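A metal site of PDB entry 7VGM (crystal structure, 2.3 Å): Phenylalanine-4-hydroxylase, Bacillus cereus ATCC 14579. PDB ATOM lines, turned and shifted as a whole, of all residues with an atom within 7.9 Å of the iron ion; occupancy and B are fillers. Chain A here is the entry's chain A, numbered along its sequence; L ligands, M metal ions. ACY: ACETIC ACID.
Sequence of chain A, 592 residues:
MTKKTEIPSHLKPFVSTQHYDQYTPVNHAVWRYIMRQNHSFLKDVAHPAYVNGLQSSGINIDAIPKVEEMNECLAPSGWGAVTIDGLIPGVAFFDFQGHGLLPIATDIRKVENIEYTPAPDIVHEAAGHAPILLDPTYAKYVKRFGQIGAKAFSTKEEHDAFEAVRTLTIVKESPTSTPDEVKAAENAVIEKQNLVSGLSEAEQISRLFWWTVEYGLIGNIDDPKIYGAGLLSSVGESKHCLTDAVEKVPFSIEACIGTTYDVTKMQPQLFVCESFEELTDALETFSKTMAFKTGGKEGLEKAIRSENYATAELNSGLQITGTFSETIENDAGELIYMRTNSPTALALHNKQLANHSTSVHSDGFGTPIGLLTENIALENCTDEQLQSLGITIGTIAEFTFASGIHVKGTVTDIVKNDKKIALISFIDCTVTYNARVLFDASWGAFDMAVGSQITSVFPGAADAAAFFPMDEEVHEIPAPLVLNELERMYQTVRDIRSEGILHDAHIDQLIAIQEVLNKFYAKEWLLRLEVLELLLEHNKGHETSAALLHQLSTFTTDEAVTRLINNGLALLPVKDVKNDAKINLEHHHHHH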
ATOM      1  N   PHE A  93     -16.840 -13.162 -10.330  1.00  0.00           N
ATOM      2  CA  PHE A  93     -17.744 -13.044  -9.166  1.00  0.00           C
ATOM      3  C   PHE A  93     -18.970 -13.942  -9.393  1.00  0.00           C
ATOM      4  O   PHE A  93     -19.314 -14.713  -8.505  1.00  0.00           O
ATOM      5  CB  PHE A  93     -18.034 -11.568  -8.899  1.00  0.00           C
ATOM      6  CG  PHE A  93     -19.208 -11.255  -7.996  1.00  0.00           C
ATOM      7  CD1 PHE A  93     -19.084 -11.336  -6.626  1.00  0.00           C
ATOM      8  CD2 PHE A  93     -20.416 -10.828  -8.532  1.00  0.00           C
ATOM      9  CE1 PHE A  93     -20.147 -11.024  -5.801  1.00  0.00           C
ATOM     10  CE2 PHE A  93     -21.478 -10.516  -7.708  1.00  0.00           C
ATOM     11  CZ  PHE A  93     -21.344 -10.614  -6.337  1.00  0.00           C
ATOM     12  N   PRO A 120     -17.653  -2.646   0.417  1.00  0.00           N
ATOM     13  CA  PRO A 120     -18.377  -3.767   1.009  1.00  0.00           C
ATOM     14  C   PRO A 120     -17.415  -4.597   1.865  1.00  0.00           C
ATOM     15  O   PRO A 120     -16.296  -4.836   1.454  1.00  0.00           O
ATOM     16  CB  PRO A 120     -18.968  -4.515  -0.195  1.00  0.00           C
ATOM     17  CG  PRO A 120     -19.005  -3.477  -1.289  1.00  0.00           C
ATOM     18  CD  PRO A 120     -17.803  -2.594  -1.040  1.00  0.00           C
ATOM     19  N   ASP A 121     -17.886  -5.009   3.034  1.00  0.00           N
ATOM     20  CA  ASP A 121     -17.034  -5.743   3.994  1.00  0.00           C
ATOM     21  C   ASP A 121     -17.635  -7.107   4.298  1.00  0.00           C
ATOM     22  O   ASP A 121     -18.592  -7.469   3.633  1.00  0.00           O
ATOM     23  CB  ASP A 121     -16.866  -4.884   5.243  1.00  0.00           C
ATOM     24  CG  ASP A 121     -18.145  -4.651   6.017  1.00  0.00           C
ATOM     25  OD1 ASP A 121     -19.228  -4.749   5.418  1.00  0.00           O
ATOM     26  OD2 ASP A 121     -18.052  -4.373   7.221  1.00  0.00           O
ATOM     27  N   HIS A 124     -21.500  -7.320   5.042  1.00  0.00           N
ATOM     28  CA  HIS A 124     -22.357  -7.443   3.836  1.00  0.00           C
ATOM     29  C   HIS A 124     -22.116  -8.751   3.092  1.00  0.00           C
ATOM     30  O   HIS A 124     -23.095  -9.386   2.734  1.00  0.00           O
ATOM     31  CB  HIS A 124     -22.158  -6.243   2.917  1.00  0.00           C
ATOM     32  CG  HIS A 124     -22.840  -6.433   1.611  1.00  0.00           C
ATOM     33  ND1 HIS A 124     -24.202  -6.351   1.485  1.00  0.00           N
ATOM     34  CD2 HIS A 124     -22.365  -6.765   0.398  1.00  0.00           C
ATOM     35  CE1 HIS A 124     -24.535  -6.593   0.247  1.00  0.00           C
ATOM     36  NE2 HIS A 124     -23.431  -6.854  -0.443  1.00  0.00           N
ATOM     37  N   GLU A 125     -20.866  -9.143   2.890  1.00  0.00           N
ATOM     38  CA  GLU A 125     -20.540 -10.290   2.011  1.00  0.00           C
ATOM     39  C   GLU A 125     -20.830 -11.632   2.683  1.00  0.00           C
ATOM     40  O   GLU A 125     -21.143 -12.569   1.970  1.00  0.00           O
ATOM     41  CB  GLU A 125     -19.145 -10.094   1.417  1.00  0.00           C
ATOM     42  CG  GLU A 125     -19.036  -8.831   0.582  1.00  0.00           C
ATOM     43  CD  GLU A 125     -17.804  -8.763  -0.294  1.00  0.00           C
ATOM     44  OE1 GLU A 125     -17.254  -9.813  -0.612  1.00  0.00           O
ATOM     45  OE2 GLU A 125     -17.398  -7.643  -0.642  1.00  0.00           O
ATOM     46  N   GLY A 128     -24.974 -10.606   4.870  1.00  0.00           N
ATOM     47  CA  GLY A 128     -26.025 -10.271   3.906  1.00  0.00           C
ATOM     48  C   GLY A 128     -26.257 -11.335   2.852  1.00  0.00           C
ATOM     49  O   GLY A 128     -27.404 -11.663   2.632  1.00  0.00           O
ATOM     50  N   HIS A 129     -25.192 -11.858   2.249  1.00  0.00           N
ATOM     51  CA  HIS A 129     -25.325 -12.778   1.081  1.00  0.00           C
ATOM     52  C   HIS A 129     -25.526 -14.278   1.423  1.00  0.00           C
ATOM     53  O   HIS A 129     -25.971 -14.980   0.528  1.00  0.00           O
ATOM     54  CB  HIS A 129     -24.127 -12.554   0.139  1.00  0.00           C
ATOM     55  CG  HIS A 129     -24.182 -11.361  -0.751  1.00  0.00           C
ATOM     56  ND1 HIS A 129     -24.681 -11.423  -2.027  1.00  0.00           N
ATOM     57  CD2 HIS A 129     -23.750 -10.102  -0.586  1.00  0.00           C
ATOM     58  CE1 HIS A 129     -24.582 -10.249  -2.596  1.00  0.00           C
ATOM     59  NE2 HIS A 129     -24.017  -9.424  -1.735  1.00  0.00           N
ATOM     60  N   PHE A 209     -29.182  -8.114 -10.601  1.00  0.00           N
ATOM     61  CA  PHE A 209     -28.575  -8.599  -9.336  1.00  0.00           C
ATOM     62  C   PHE A 209     -28.854  -7.598  -8.212  1.00  0.00           C
ATOM     63  O   PHE A 209     -29.235  -8.037  -7.138  1.00  0.00           O
ATOM     64  CB  PHE A 209     -27.076  -8.821  -9.534  1.00  0.00           C
ATOM     65  CG  PHE A 209     -26.350  -9.622  -8.492  1.00  0.00           C
ATOM     66  CD1 PHE A 209     -26.469 -11.001  -8.443  1.00  0.00           C
ATOM     67  CD2 PHE A 209     -25.529  -9.002  -7.570  1.00  0.00           C
ATOM     68  CE1 PHE A 209     -25.784 -11.734  -7.492  1.00  0.00           C
ATOM     69  CE2 PHE A 209     -24.853  -9.741  -6.618  1.00  0.00           C
ATOM     70  CZ  PHE A 209     -24.983 -11.103  -6.579  1.00  0.00           C
ATOM     71  N   TRP A 210     -28.678  -6.291  -8.482  1.00  0.00           N
ATOM     72  CA  TRP A 210     -28.915  -5.228  -7.485  1.00  0.00           C
ATOM     73  C   TRP A 210     -30.363  -5.222  -6.968  1.00  0.00           C
ATOM     74  O   TRP A 210     -30.529  -5.097  -5.768  1.00  0.00           O
ATOM     75  CB  TRP A 210     -28.529  -3.872  -8.064  1.00  0.00           C
ATOM     76  CG  TRP A 210     -28.610  -2.723  -7.103  1.00  0.00           C
ATOM     77  CD1 TRP A 210     -29.665  -1.876  -6.928  1.00  0.00           C
ATOM     78  CD2 TRP A 210     -27.586  -2.293  -6.195  1.00  0.00           C
ATOM     79  NE1 TRP A 210     -29.368  -0.948  -5.973  1.00  0.00           N
ATOM     80  CE2 TRP A 210     -28.105  -1.174  -5.502  1.00  0.00           C
ATOM     81  CE3 TRP A 210     -26.296  -2.740  -5.895  1.00  0.00           C
ATOM     82  CZ2 TRP A 210     -27.363  -0.497  -4.536  1.00  0.00           C
ATOM     83  CZ3 TRP A 210     -25.572  -2.074  -4.948  1.00  0.00           C
ATOM     84  CH2 TRP A 210     -26.095  -0.970  -4.273  1.00  0.00           C
ATOM     85  N   VAL A 213     -30.844  -9.977  -5.647  1.00  0.00           N
ATOM     86  CA  VAL A 213     -29.877 -10.471  -4.638  1.00  0.00           C
ATOM     87  C   VAL A 213     -29.470  -9.390  -3.628  1.00  0.00           C
ATOM     88  O   VAL A 213     -29.312  -9.747  -2.467  1.00  0.00           O
ATOM     89  CB  VAL A 213     -28.690 -11.130  -5.354  1.00  0.00           C
ATOM     90  CG1 VAL A 213     -27.742 -11.827  -4.393  1.00  0.00           C
ATOM     91  CG2 VAL A 213     -29.178 -12.109  -6.413  1.00  0.00           C
ATOM     92  N   GLU A 214     -29.358  -8.136  -4.042  1.00  0.00           N
ATOM     93  CA  GLU A 214     -28.846  -7.037  -3.171  1.00  0.00           C
ATOM     94  C   GLU A 214     -29.927  -6.227  -2.451  1.00  0.00           C
ATOM     95  O   GLU A 214     -29.736  -5.959  -1.274  1.00  0.00           O
ATOM     96  CB  GLU A 214     -27.973  -6.119  -4.025  1.00  0.00           C
ATOM     97  CG  GLU A 214     -26.799  -6.822  -4.677  1.00  0.00           C
ATOM     98  CD  GLU A 214     -25.661  -7.089  -3.722  1.00  0.00           C
ATOM     99  OE1 GLU A 214     -25.822  -6.807  -2.530  1.00  0.00           O
ATOM    100  OE2 GLU A 214     -24.611  -7.562  -4.176  1.00  0.00           O
ATOM    101  N   TYR A 215     -30.991  -5.805  -3.128  1.00  0.00           N
ATOM    102  CA  TYR A 215     -32.015  -4.901  -2.537  1.00  0.00           C
ATOM    103  C   TYR A 215     -33.430  -5.457  -2.727  1.00  0.00           C
ATOM    104  O   TYR A 215     -34.386  -4.690  -2.666  1.00  0.00           O
ATOM    105  CB  TYR A 215     -31.737  -3.459  -2.952  1.00  0.00           C
ATOM    106  CG  TYR A 215     -30.602  -2.816  -2.184  1.00  0.00           C
ATOM    107  CD1 TYR A 215     -30.842  -2.146  -0.996  1.00  0.00           C
ATOM    108  CD2 TYR A 215     -29.300  -2.915  -2.615  1.00  0.00           C
ATOM    109  CE1 TYR A 215     -29.820  -1.577  -0.276  1.00  0.00           C
ATOM    110  CE2 TYR A 215     -28.259  -2.357  -1.896  1.00  0.00           C
ATOM    111  CZ  TYR A 215     -28.520  -1.677  -0.727  1.00  0.00           C
ATOM    112  OH  TYR A 215     -27.494  -1.116  -0.027  1.00  0.00           O
ATOM    113  N   GLY A 228     -32.892  -9.035   0.348  1.00  0.00           N
ATOM    114  CA  GLY A 228     -31.698  -8.409  -0.233  1.00  0.00           C
ATOM    115  C   GLY A 228     -30.521  -8.308   0.710  1.00  0.00           C
ATOM    116  O   GLY A 228     -30.709  -7.830   1.804  1.00  0.00           O
ATOM    117  N   ALA A 229     -29.348  -8.715   0.244  1.00  0.00           N
ATOM    118  CA  ALA A 229     -28.107  -8.716   1.067  1.00  0.00           C
ATOM    119  C   ALA A 229     -27.759  -7.320   1.613  1.00  0.00           C
ATOM    120  O   ALA A 229     -27.379  -7.239   2.776  1.00  0.00           O
ATOM    121  CB  ALA A 229     -26.999  -9.319   0.274  1.00  0.00           C
ATOM    122  N   GLY A 230     -27.873  -6.282   0.805  1.00  0.00           N
ATOM    123  CA  GLY A 230     -27.620  -4.899   1.269  1.00  0.00           C
ATOM    124  C   GLY A 230     -28.555  -4.480   2.370  1.00  0.00           C
ATOM    125  O   GLY A 230     -28.126  -3.754   3.255  1.00  0.00           O
ATOM    126  N   SER A 233     -27.693  -6.489   5.672  1.00  0.00           N
ATOM    127  CA  SER A 233     -26.448  -5.967   6.298  1.00  0.00           C
ATOM    128  C   SER A 233     -26.629  -4.528   6.820  1.00  0.00           C
ATOM    129  O   SER A 233     -25.711  -4.048   7.481  1.00  0.00           O
ATOM    130  CB  SER A 233     -25.308  -6.089   5.327  1.00  0.00           C
ATOM    131  OG  SER A 233     -25.560  -5.342   4.153  1.00  0.00           O
HETATM  132  C   ACY L   1     -20.358  -8.574  -2.979  1.00  0.00           C
HETATM  133  O   ACY L   1     -19.504  -7.713  -3.226  1.00  0.00           O
HETATM  134  OXT ACY L   1     -21.494  -8.311  -2.689  1.00  0.00           O
HETATM  135  CH3 ACY L   1     -19.935 -10.048  -3.095  1.00  0.00           C
HETATM  136  C   ACY L   2     -22.790  -4.267  -3.151  1.00  0.00           C
HETATM  137  O   ACY L   2     -22.709  -3.973  -4.337  1.00  0.00           O
HETATM  138  OXT ACY L   2     -22.885  -5.404  -2.775  1.00  0.00           O
HETATM  139  CH3 ACY L   2     -22.754  -3.162  -2.126  1.00  0.00           C
HETATM  140 FE    FE M   1     -23.508  -7.456  -2.204  1.00  0.00          FE
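ND1 of His 124 sits at hydrogen-bond distance from OG of Ser 233 (3.2 Å). N of His 124 lies within hydrogen-bond range of OD1 of Asp 121 (3.5 Å). N of Ala 229 is in hydrogen-bond range of O of Glu 214 (3.2 Å). The backbone NH (N) of Glu 214 sits at hydrogen-bond distance from the backbone carbonyl oxygen (O) of Phe 209 (3.1 Å). O of Glu 214 sits at hydrogen-bond distance from N of Gly 230, 2.8 Å away.
Within 4 Å of the iron ion: His 124, His 129 and Glu 214.
The iron ion is bound by NE2 of His 124 (1.9 Å), NE2 of His 129 (2.1 Å), OXT of ACY L2 (2.2 Å), OXT of ACY L1 (2.2 Å), OE2 of Glu 214 (2.3 Å) and OE1 of Glu 214 (2.4 Å).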
